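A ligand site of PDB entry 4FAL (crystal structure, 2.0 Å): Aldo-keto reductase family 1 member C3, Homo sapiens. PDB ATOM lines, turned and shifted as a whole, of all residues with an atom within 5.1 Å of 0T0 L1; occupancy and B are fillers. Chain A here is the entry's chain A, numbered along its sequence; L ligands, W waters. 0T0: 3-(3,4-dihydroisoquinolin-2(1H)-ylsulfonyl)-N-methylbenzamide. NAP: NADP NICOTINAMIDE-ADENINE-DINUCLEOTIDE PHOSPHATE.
Water W1 lies within hydrogen-bond range of the side-chain hydroxyl of Ser 87, the side-chain hydroxyl of Ser 118, the backbone carbonyl oxygen of Met 120 and an oxygen (OAD) of 0T0 L1.
The side-chain hydroxyl (OH) of Tyr 55 lies within hydrogen-bond range of an oxygen (OAB) of 0T0 L1 (2.7 Å).
OAB of 0T0 L1 lies within hydrogen-bond range of NE2 of His 117, at 2.9 Å.
ND2 of Asn 167 lies within hydrogen-bond range of OAC of 0T0 L1.
A ring nitrogen (NE2) of His 117 lies within hydrogen-bond range of an oxygen (O7N) of NAP L2, 3.4 Å away.
ND2 of Asn 167 is in hydrogen-bond range of O7N of NAP L2 (2.9 Å).
The backbone NH (N) of Tyr 24 lies within hydrogen-bond range of an oxygen (O3D) of NAP L2 (3.2 Å).
ND2 of Asn 167 lies within hydrogen-bond range of O of His 117, 2.8 Å away.
N of Asn 307 sits at hydrogen-bond distance from O of Trp 227 (3.0 Å).
The side-chain amide oxygen of Asn 167 sits at hydrogen-bond distance from the side-chain hydroxyl of Tyr 216 (2.6 Å).
N of Met 120 sits at hydrogen-bond distance from OG of Ser 118.
O of Phe 306 is in hydrogen-bond range of ND1 of His 304 (2.7 Å).
Tyr 24 touches 0T0 L1 (CG to CAA, 3.5 Å).
Leu 54 touches 0T0 L1.
CH2 of Trp 86 touches OAD of 0T0 L1, at 3.4 Å.
CB of Ser 118 touches OAC of 0T0 L1, 3.4 Å away.
Met 120 touches 0T0 L1.
Tyr 216 touches 0T0 L1.
CZ2 of Trp 227 touches CAG of 0T0 L1, at 3.4 Å.
Phe 306 touches 0T0 L1.
CB of Phe 311 touches CAK of 0T0 L1, at 3.4 Å.
CE1 of Tyr 317 touches CAE of 0T0 L1, 3.4 Å away.
CE2 of Tyr 319 touches CAJ of 0T0 L1, 3.5 Å away.
Hydrophobic or aromatic side chains that line 0T0 L1: Tyr 24, Leu 54, Tyr 55, Trp 86, His 117, Met 120, Trp 227, Phe 311, Tyr 317 and Tyr 319.
Of the 19 residues printed, 14 come within 4 Å of 0T0 L1.
The nearest printed residue that does not touch 0T0 L1 is Ser 308 (4.4 Å).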
ATOM      1  N   TYR A  24       3.911 -20.062 -23.316  1.00  0.00           N
ATOM      2  CA  TYR A  24       5.186 -19.407 -22.906  1.00  0.00           C
ATOM      3  C   TYR A  24       5.790 -20.042 -21.627  1.00  0.00           C
ATOM      4  O   TYR A  24       5.085 -20.248 -20.623  1.00  0.00           O
ATOM      5  CB  TYR A  24       5.087 -17.909 -22.688  1.00  0.00           C
ATOM      6  CG  TYR A  24       6.488 -17.333 -22.327  1.00  0.00           C
ATOM      7  CD1 TYR A  24       7.486 -17.288 -23.300  1.00  0.00           C
ATOM      8  CD2 TYR A  24       6.813 -16.935 -21.026  1.00  0.00           C
ATOM      9  CE1 TYR A  24       8.762 -16.833 -23.023  1.00  0.00           C
ATOM     10  CE2 TYR A  24       8.087 -16.465 -20.718  1.00  0.00           C
ATOM     11  CZ  TYR A  24       9.067 -16.439 -21.746  1.00  0.00           C
ATOM     12  OH  TYR A  24      10.322 -15.990 -21.530  1.00  0.00           O
ATOM     13  N   LEU A  54       8.476 -14.661 -30.339  1.00  0.00           N
ATOM     14  CA  LEU A  54       9.219 -14.359 -29.100  1.00  0.00           C
ATOM     15  C   LEU A  54       9.472 -15.588 -28.200  1.00  0.00           C
ATOM     16  O   LEU A  54      10.478 -15.687 -27.526  1.00  0.00           O
ATOM     17  CB  LEU A  54       8.466 -13.291 -28.282  1.00  0.00           C
ATOM     18  CG  LEU A  54       9.230 -12.680 -27.086  1.00  0.00           C
ATOM     19  CD1 LEU A  54      10.614 -11.981 -27.483  1.00  0.00           C
ATOM     20  CD2 LEU A  54       8.366 -11.695 -26.240  1.00  0.00           C
ATOM     21  N   TYR A  55       8.517 -16.481 -28.169  1.00  0.00           N
ATOM     22  CA  TYR A  55       8.512 -17.612 -27.220  1.00  0.00           C
ATOM     23  C   TYR A  55       9.564 -18.688 -27.531  1.00  0.00           C
ATOM     24  O   TYR A  55       9.818 -19.573 -26.665  1.00  0.00           O
ATOM     25  CB  TYR A  55       7.143 -18.232 -27.066  1.00  0.00           C
ATOM     26  CG  TYR A  55       6.027 -17.257 -26.655  1.00  0.00           C
ATOM     27  CD1 TYR A  55       6.310 -15.968 -26.222  1.00  0.00           C
ATOM     28  CD2 TYR A  55       4.690 -17.618 -26.761  1.00  0.00           C
ATOM     29  CE1 TYR A  55       5.290 -15.064 -25.953  1.00  0.00           C
ATOM     30  CE2 TYR A  55       3.666 -16.753 -26.443  1.00  0.00           C
ATOM     31  CZ  TYR A  55       3.977 -15.465 -26.034  1.00  0.00           C
ATOM     32  OH  TYR A  55       3.035 -14.511 -25.740  1.00  0.00           O
ATOM     33  N   TRP A  86       6.765 -10.226 -33.837  1.00  0.00           N
ATOM     34  CA  TRP A  86       7.545  -9.591 -32.816  1.00  0.00           C
ATOM     35  C   TRP A  86       7.859  -8.120 -33.210  1.00  0.00           C
ATOM     36  O   TRP A  86       7.793  -7.744 -34.368  1.00  0.00           O
ATOM     37  CB  TRP A  86       8.815 -10.445 -32.422  1.00  0.00           C
ATOM     38  CG  TRP A  86       9.562  -9.793 -31.321  1.00  0.00           C
ATOM     39  CD1 TRP A  86      10.850  -9.360 -31.356  1.00  0.00           C
ATOM     40  CD2 TRP A  86       9.020  -9.294 -30.082  1.00  0.00           C
ATOM     41  NE1 TRP A  86      11.185  -8.726 -30.192  1.00  0.00           N
ATOM     42  CE2 TRP A  86      10.065  -8.620 -29.411  1.00  0.00           C
ATOM     43  CE3 TRP A  86       7.781  -9.375 -29.468  1.00  0.00           C
ATOM     44  CZ2 TRP A  86       9.902  -8.054 -28.138  1.00  0.00           C
ATOM     45  CZ3 TRP A  86       7.622  -8.767 -28.170  1.00  0.00           C
ATOM     46  CH2 TRP A  86       8.674  -8.117 -27.571  1.00  0.00           C
ATOM     47  N   SER A  87       8.122  -7.298 -32.221  1.00  0.00           N
ATOM     48  CA  SER A  87       8.155  -5.830 -32.339  1.00  0.00           C
ATOM     49  C   SER A  87       9.350  -5.235 -33.133  1.00  0.00           C
ATOM     50  O   SER A  87       9.327  -4.072 -33.502  1.00  0.00           O
ATOM     51  CB  SER A  87       8.069  -5.241 -30.909  1.00  0.00           C
ATOM     52  OG  SER A  87       6.853  -5.702 -30.296  1.00  0.00           O
ATOM     53  N   HIS A 117       2.214  -8.382 -31.833  1.00  0.00           N
ATOM     54  CA  HIS A 117       2.445  -8.750 -30.452  1.00  0.00           C
ATOM     55  C   HIS A 117       2.287  -7.545 -29.490  1.00  0.00           C
ATOM     56  O   HIS A 117       1.849  -7.695 -28.350  1.00  0.00           O
ATOM     57  CB  HIS A 117       3.855  -9.366 -30.317  1.00  0.00           C
ATOM     58  CG  HIS A 117       4.045 -10.237 -29.130  1.00  0.00           C
ATOM     59  ND1 HIS A 117       4.872 -11.353 -29.171  1.00  0.00           N
ATOM     60  CD2 HIS A 117       3.633 -10.130 -27.838  1.00  0.00           C
ATOM     61  CE1 HIS A 117       4.899 -11.917 -27.975  1.00  0.00           C
ATOM     62  NE2 HIS A 117       4.141 -11.198 -27.153  1.00  0.00           N
ATOM     63  N   SER A 118       2.675  -6.346 -29.950  1.00  0.00           N
ATOM     64  CA  SER A 118       2.781  -5.162 -29.090  1.00  0.00           C
ATOM     65  C   SER A 118       2.860  -3.942 -29.993  1.00  0.00           C
ATOM     66  O   SER A 118       3.444  -4.034 -31.078  1.00  0.00           O
ATOM     67  CB  SER A 118       4.053  -5.256 -28.270  1.00  0.00           C
ATOM     68  OG  SER A 118       4.518  -4.022 -27.736  1.00  0.00           O
ATOM     69  N   MET A 120       4.741  -1.505 -29.228  1.00  0.00           N
ATOM     70  CA  MET A 120       5.982  -0.844 -28.867  1.00  0.00           C
ATOM     71  C   MET A 120       7.091  -1.283 -29.797  1.00  0.00           C
ATOM     72  O   MET A 120       7.920  -2.174 -29.496  1.00  0.00           O
ATOM     73  CB  MET A 120       6.282  -1.018 -27.399  1.00  0.00           C
ATOM     74  CG  MET A 120       5.143  -0.465 -26.433  1.00  0.00           C
ATOM     75  SD  MET A 120       5.604  -0.767 -24.731  1.00  0.00           S
ATOM     76  CE  MET A 120       5.228  -2.525 -24.667  1.00  0.00           C
ATOM     77  N   ASN A 167      -1.766  -6.025 -26.805  1.00  0.00           N
ATOM     78  CA  ASN A 167      -1.264  -4.961 -26.017  1.00  0.00           C
ATOM     79  C   ASN A 167      -1.624  -3.536 -26.527  1.00  0.00           C
ATOM     80  O   ASN A 167      -0.943  -2.576 -26.180  1.00  0.00           O
ATOM     81  CB  ASN A 167       0.228  -5.126 -25.796  1.00  0.00           C
ATOM     82  CG  ASN A 167       0.532  -6.336 -25.023  1.00  0.00           C
ATOM     83  OD1 ASN A 167       0.060  -6.465 -23.862  1.00  0.00           O
ATOM     84  ND2 ASN A 167       1.321  -7.241 -25.590  1.00  0.00           N
ATOM     85  N   TYR A 216      -4.614 -12.339 -21.320  1.00  0.00           N
ATOM     86  CA  TYR A 216      -3.409 -13.064 -20.884  1.00  0.00           C
ATOM     87  C   TYR A 216      -3.057 -12.684 -19.460  1.00  0.00           C
ATOM     88  O   TYR A 216      -3.494 -11.685 -18.928  1.00  0.00           O
ATOM     89  CB  TYR A 216      -2.220 -12.810 -21.830  1.00  0.00           C
ATOM     90  CG  TYR A 216      -1.529 -11.450 -21.775  1.00  0.00           C
ATOM     91  CD1 TYR A 216      -0.774 -11.067 -20.718  1.00  0.00           C
ATOM     92  CD2 TYR A 216      -1.557 -10.594 -22.874  1.00  0.00           C
ATOM     93  CE1 TYR A 216      -0.137  -9.874 -20.692  1.00  0.00           C
ATOM     94  CE2 TYR A 216      -0.908  -9.393 -22.851  1.00  0.00           C
ATOM     95  CZ  TYR A 216      -0.196  -9.035 -21.790  1.00  0.00           C
ATOM     96  OH  TYR A 216       0.517  -7.823 -21.720  1.00  0.00           O
ATOM     97  N   TRP A 227      10.349  -8.882 -15.539  1.00  0.00           N
ATOM     98  CA  TRP A 227       9.236  -7.985 -15.891  1.00  0.00           C
ATOM     99  C   TRP A 227       8.324  -7.658 -14.714  1.00  0.00           C
ATOM    100  O   TRP A 227       7.557  -6.679 -14.818  1.00  0.00           O
ATOM    101  CB  TRP A 227       8.363  -8.647 -17.004  1.00  0.00           C
ATOM    102  CG  TRP A 227       9.139  -8.968 -18.226  1.00  0.00           C
ATOM    103  CD1 TRP A 227       9.829  -8.095 -18.972  1.00  0.00           C
ATOM    104  CD2 TRP A 227       9.289 -10.245 -18.826  1.00  0.00           C
ATOM    105  NE1 TRP A 227      10.452  -8.754 -20.029  1.00  0.00           N
ATOM    106  CE2 TRP A 227      10.123 -10.080 -19.966  1.00  0.00           C
ATOM    107  CE3 TRP A 227       8.757 -11.497 -18.557  1.00  0.00           C
ATOM    108  CZ2 TRP A 227      10.470 -11.148 -20.818  1.00  0.00           C
ATOM    109  CZ3 TRP A 227       9.095 -12.599 -19.432  1.00  0.00           C
ATOM    110  CH2 TRP A 227       9.959 -12.402 -20.540  1.00  0.00           C
ATOM    111  N   HIS A 304      -1.119  -3.922 -13.359  1.00  0.00           N
ATOM    112  CA  HIS A 304      -0.507  -4.675 -14.399  1.00  0.00           C
ATOM    113  C   HIS A 304       0.809  -5.314 -13.916  1.00  0.00           C
ATOM    114  O   HIS A 304       1.695  -4.651 -13.321  1.00  0.00           O
ATOM    115  CB  HIS A 304      -0.331  -3.867 -15.665  1.00  0.00           C
ATOM    116  CG  HIS A 304       0.369  -2.544 -15.467  1.00  0.00           C
ATOM    117  ND1 HIS A 304       1.718  -2.387 -15.662  1.00  0.00           N
ATOM    118  CD2 HIS A 304      -0.097  -1.324 -15.099  1.00  0.00           C
ATOM    119  CE1 HIS A 304       2.059  -1.118 -15.420  1.00  0.00           C
ATOM    120  NE2 HIS A 304       0.959  -0.459 -15.076  1.00  0.00           N
ATOM    121  N   PHE A 306       3.150  -6.753 -15.804  1.00  0.00           N
ATOM    122  CA  PHE A 306       4.263  -6.294 -16.623  1.00  0.00           C
ATOM    123  C   PHE A 306       4.500  -4.826 -16.284  1.00  0.00           C
ATOM    124  O   PHE A 306       3.682  -3.971 -16.600  1.00  0.00           O
ATOM    125  CB  PHE A 306       4.003  -6.462 -18.101  1.00  0.00           C
ATOM    126  CG  PHE A 306       4.171  -7.887 -18.603  1.00  0.00           C
ATOM    127  CD1 PHE A 306       5.322  -8.242 -19.322  1.00  0.00           C
ATOM    128  CD2 PHE A 306       3.262  -8.859 -18.288  1.00  0.00           C
ATOM    129  CE1 PHE A 306       5.493  -9.560 -19.777  1.00  0.00           C
ATOM    130  CE2 PHE A 306       3.447 -10.193 -18.697  1.00  0.00           C
ATOM    131  CZ  PHE A 306       4.560 -10.534 -19.462  1.00  0.00           C
ATOM    132  N   ASN A 307       5.626  -4.539 -15.640  1.00  0.00           N
ATOM    133  CA  ASN A 307       5.869  -3.219 -15.146  1.00  0.00           C
ATOM    134  C   ASN A 307       7.379  -3.009 -15.118  1.00  0.00           C
ATOM    135  O   ASN A 307       8.052  -3.218 -14.065  1.00  0.00           O
ATOM    136  CB  ASN A 307       5.194  -3.098 -13.768  1.00  0.00           C
ATOM    137  CG  ASN A 307       5.441  -1.760 -13.080  1.00  0.00           C
ATOM    138  OD1 ASN A 307       5.771  -0.793 -13.716  1.00  0.00           O
ATOM    139  ND2 ASN A 307       5.307  -1.731 -11.743  1.00  0.00           N
ATOM    140  N   SER A 308       7.927  -2.631 -16.293  1.00  0.00           N
ATOM    141  CA  SER A 308       9.369  -2.544 -16.472  1.00  0.00           C
ATOM    142  C   SER A 308       9.860  -1.231 -17.081  1.00  0.00           C
ATOM    143  O   SER A 308       9.227  -0.645 -17.997  1.00  0.00           O
ATOM    144  CB  SER A 308       9.858  -3.733 -17.278  1.00  0.00           C
ATOM    145  OG  SER A 308      11.228  -3.662 -17.547  1.00  0.00           O
ATOM    146  N   PHE A 311      10.029  -0.883 -20.958  1.00  0.00           N
ATOM    147  CA  PHE A 311       8.944  -0.365 -21.758  1.00  0.00           C
ATOM    148  C   PHE A 311       8.134   0.852 -21.287  1.00  0.00           C
ATOM    149  O   PHE A 311       7.397   1.410 -22.106  1.00  0.00           O
ATOM    150  CB  PHE A 311       8.051  -1.518 -22.109  1.00  0.00           C
ATOM    151  CG  PHE A 311       8.670  -2.446 -23.191  1.00  0.00           C
ATOM    152  CD1 PHE A 311       8.959  -1.931 -24.493  1.00  0.00           C
ATOM    153  CD2 PHE A 311       8.985  -3.760 -22.909  1.00  0.00           C
ATOM    154  CE1 PHE A 311       9.525  -2.765 -25.512  1.00  0.00           C
ATOM    155  CE2 PHE A 311       9.590  -4.617 -23.934  1.00  0.00           C
ATOM    156  CZ  PHE A 311       9.827  -4.118 -25.244  1.00  0.00           C
ATOM    157  N   TYR A 317       3.861   3.088 -25.346  1.00  0.00           N
ATOM    158  CA  TYR A 317       3.414   2.374 -24.124  1.00  0.00           C
ATOM    159  C   TYR A 317       1.896   2.400 -23.992  1.00  0.00           C
ATOM    160  O   TYR A 317       1.307   3.458 -23.973  1.00  0.00           O
ATOM    161  CB  TYR A 317       4.112   3.025 -22.948  1.00  0.00           C
ATOM    162  CG  TYR A 317       3.900   2.391 -21.615  1.00  0.00           C
ATOM    163  CD1 TYR A 317       4.338   1.111 -21.369  1.00  0.00           C
ATOM    164  CD2 TYR A 317       3.316   3.108 -20.558  1.00  0.00           C
ATOM    165  CE1 TYR A 317       4.201   0.500 -20.088  1.00  0.00           C
ATOM    166  CE2 TYR A 317       3.203   2.513 -19.245  1.00  0.00           C
ATOM    167  CZ  TYR A 317       3.623   1.201 -19.049  1.00  0.00           C
ATOM    168  OH  TYR A 317       3.499   0.538 -17.852  1.00  0.00           O
ATOM    169  N   PRO A 318       1.235   1.210 -23.869  1.00  0.00           N
ATOM    170  CA  PRO A 318      -0.172   1.172 -23.831  1.00  0.00           C
ATOM    171  C   PRO A 318      -0.812   1.706 -22.580  1.00  0.00           C
ATOM    172  O   PRO A 318      -1.981   2.022 -22.635  1.00  0.00           O
ATOM    173  CB  PRO A 318      -0.520  -0.324 -24.003  1.00  0.00           C
ATOM    174  CG  PRO A 318       0.589  -1.035 -23.602  1.00  0.00           C
ATOM    175  CD  PRO A 318       1.803  -0.160 -23.882  1.00  0.00           C
ATOM    176  N   TYR A 319      -0.100   1.753 -21.468  1.00  0.00           N
ATOM    177  CA  TYR A 319      -0.731   2.064 -20.212  1.00  0.00           C
ATOM    178  C   TYR A 319      -0.580   3.532 -19.838  1.00  0.00           C
ATOM    179  O   TYR A 319      -0.959   3.894 -18.748  1.00  0.00           O
ATOM    180  CB  TYR A 319      -0.195   1.170 -19.079  1.00  0.00           C
ATOM    181  CG  TYR A 319      -0.407  -0.292 -19.343  1.00  0.00           C
ATOM    182  CD1 TYR A 319      -1.548  -0.773 -19.964  1.00  0.00           C
ATOM    183  CD2 TYR A 319       0.536  -1.209 -18.932  1.00  0.00           C
ATOM    184  CE1 TYR A 319      -1.722  -2.158 -20.218  1.00  0.00           C
ATOM    185  CE2 TYR A 319       0.340  -2.570 -19.146  1.00  0.00           C
ATOM    186  CZ  TYR A 319      -0.771  -3.020 -19.774  1.00  0.00           C
ATOM    187  OH  TYR A 319      -0.897  -4.384 -19.959  1.00  0.00           O
HETATM  188  CAN 0T0 L   1       3.628  -6.562 -23.011  1.00  0.00           C
HETATM  189  CAM 0T0 L   1       2.956  -5.268 -22.487  1.00  0.00           C
HETATM  190  CAT 0T0 L   1       3.826  -4.507 -21.601  1.00  0.00           C
HETATM  191  CAJ 0T0 L   1       3.203  -3.600 -20.788  1.00  0.00           C
HETATM  192  CAE 0T0 L   1       4.035  -2.867 -19.923  1.00  0.00           C
HETATM  193  CAF 0T0 L   1       5.433  -2.998 -19.886  1.00  0.00           C
HETATM  194  CAK 0T0 L   1       6.061  -3.915 -20.738  1.00  0.00           C
HETATM  195  CAU 0T0 L   1       5.209  -4.651 -21.590  1.00  0.00           C
HETATM  196  CAO 0T0 L   1       5.935  -5.619 -22.524  1.00  0.00           C
HETATM  197  NAV 0T0 L   1       5.093  -6.628 -23.153  1.00  0.00           N
HETATM  198  SAW 0T0 L   1       5.786  -7.183 -24.721  1.00  0.00           S
HETATM  199  OAC 0T0 L   1       4.744  -7.470 -25.743  1.00  0.00           O
HETATM  200  OAD 0T0 L   1       6.842  -6.315 -25.295  1.00  0.00           O
HETATM  201  CAS 0T0 L   1       6.480  -8.678 -24.124  1.00  0.00           C
HETATM  202  CAL 0T0 L   1       5.662  -9.820 -24.154  1.00  0.00           C
HETATM  203  CAI 0T0 L   1       7.755  -8.638 -23.560  1.00  0.00           C
HETATM  204  CAG 0T0 L   1       8.229  -9.842 -23.049  1.00  0.00           C
HETATM  205  CAH 0T0 L   1       7.455 -11.015 -23.089  1.00  0.00           C
HETATM  206  CAR 0T0 L   1       6.157 -11.033 -23.651  1.00  0.00           C
HETATM  207  CAQ 0T0 L   1       5.289 -12.298 -23.685  1.00  0.00           C
HETATM  208  OAB 0T0 L   1       4.418 -12.521 -24.583  1.00  0.00           O
HETATM  209  NAP 0T0 L   1       5.576 -13.174 -22.701  1.00  0.00           N
HETATM  210  CAA 0T0 L   1       4.678 -14.376 -22.726  1.00  0.00           C
HETATM  211  PA  NAP L   2      -0.950 -17.366 -16.590  1.00  0.00           P
HETATM  212  O1A NAP L   2      -1.921 -18.016 -17.484  1.00  0.00           O
HETATM  213  O2A NAP L   2      -1.314 -16.114 -15.878  1.00  0.00           O
HETATM  214  O5B NAP L   2      -0.483 -18.496 -15.518  1.00  0.00           O
HETATM  215  C5B NAP L   2       0.404 -18.089 -14.524  1.00  0.00           C
HETATM  216  C4B NAP L   2       0.833 -19.355 -13.639  1.00  0.00           C
HETATM  217  O4B NAP L   2      -0.387 -19.928 -13.222  1.00  0.00           O
HETATM  218  C3B NAP L   2       1.459 -20.386 -14.555  1.00  0.00           C
HETATM  219  O3B NAP L   2       2.867 -20.192 -14.592  1.00  0.00           O
HETATM  220  C2B NAP L   2       0.973 -21.715 -13.964  1.00  0.00           C
HETATM  221  O2B NAP L   2       2.041 -22.308 -13.225  1.00  0.00           O
HETATM  222  C1B NAP L   2      -0.139 -21.316 -12.985  1.00  0.00           C
HETATM  223  N9A NAP L   2      -1.406 -22.133 -13.100  1.00  0.00           N
HETATM  224  C8A NAP L   2      -2.042 -22.562 -14.177  1.00  0.00           C
HETATM  225  N7A NAP L   2      -3.144 -23.220 -13.851  1.00  0.00           N
HETATM  226  C5A NAP L   2      -3.170 -23.243 -12.532  1.00  0.00           C
HETATM  227  C6A NAP L   2      -4.049 -23.836 -11.607  1.00  0.00           C
HETATM  228  N6A NAP L   2      -5.154 -24.505 -11.998  1.00  0.00           N
HETATM  229  N1A NAP L   2      -3.822 -23.627 -10.294  1.00  0.00           N
HETATM  230  C2A NAP L   2      -2.639 -22.983  -9.700  1.00  0.00           C
HETATM  231  N3A NAP L   2      -1.815 -22.383 -10.718  1.00  0.00           N
HETATM  232  C4A NAP L   2      -2.079 -22.540 -12.081  1.00  0.00           C
HETATM  233  O3  NAP L   2       0.404 -17.212 -17.346  1.00  0.00           O
HETATM  234  PN  NAP L   2       0.976 -16.234 -18.491  1.00  0.00           P
HETATM  235  O1N NAP L   2       2.122 -16.982 -19.180  1.00  0.00           O
HETATM  236  O2N NAP L   2       1.259 -14.904 -17.912  1.00  0.00           O
HETATM  237  O5D NAP L   2      -0.277 -16.053 -19.451  1.00  0.00           O
HETATM  238  C5D NAP L   2      -0.715 -17.061 -20.351  1.00  0.00           C
HETATM  239  C4D NAP L   2      -0.332 -16.957 -21.858  1.00  0.00           C
HETATM  240  O4D NAP L   2      -0.686 -15.684 -22.364  1.00  0.00           O
HETATM  241  C3D NAP L   2       1.161 -16.987 -22.065  1.00  0.00           C
HETATM  242  O3D NAP L   2       1.659 -18.338 -21.868  1.00  0.00           O
HETATM  243  C2D NAP L   2       1.280 -16.587 -23.518  1.00  0.00           C
HETATM  244  O2D NAP L   2       0.745 -17.608 -24.358  1.00  0.00           O
HETATM  245  C1D NAP L   2       0.260 -15.432 -23.419  1.00  0.00           C
HETATM  246  N1N NAP L   2       0.850 -14.152 -23.085  1.00  0.00           N
HETATM  247  C2N NAP L   2       0.889 -13.168 -24.036  1.00  0.00           C
HETATM  248  C3N NAP L   2       1.468 -11.905 -23.790  1.00  0.00           C
HETATM  249  C7N NAP L   2       1.470 -10.884 -24.861  1.00  0.00           C
HETATM  250  O7N NAP L   2       2.173  -9.860 -24.738  1.00  0.00           O
HETATM  251  N7N NAP L   2       0.528 -11.046 -25.783  1.00  0.00           N
HETATM  252  C4N NAP L   2       2.012 -11.618 -22.526  1.00  0.00           C
HETATM  253  C5N NAP L   2       1.876 -12.623 -21.531  1.00  0.00           C
HETATM  254  C6N NAP L   2       1.315 -13.850 -21.787  1.00  0.00           C
HETATM  255  P2B NAP L   2       2.336 -23.911 -13.681  1.00  0.00           P
HETATM  256  O1X NAP L   2       2.958 -23.809 -15.072  1.00  0.00           O
HETATM  257  O2X NAP L   2       3.357 -24.374 -12.660  1.00  0.00           O
HETATM  258  O3X NAP L   2       0.943 -24.677 -13.691  1.00  0.00           O
HETATM  259  O   HOH W   1       7.249  -4.543 -27.928  1.00  0.00           O
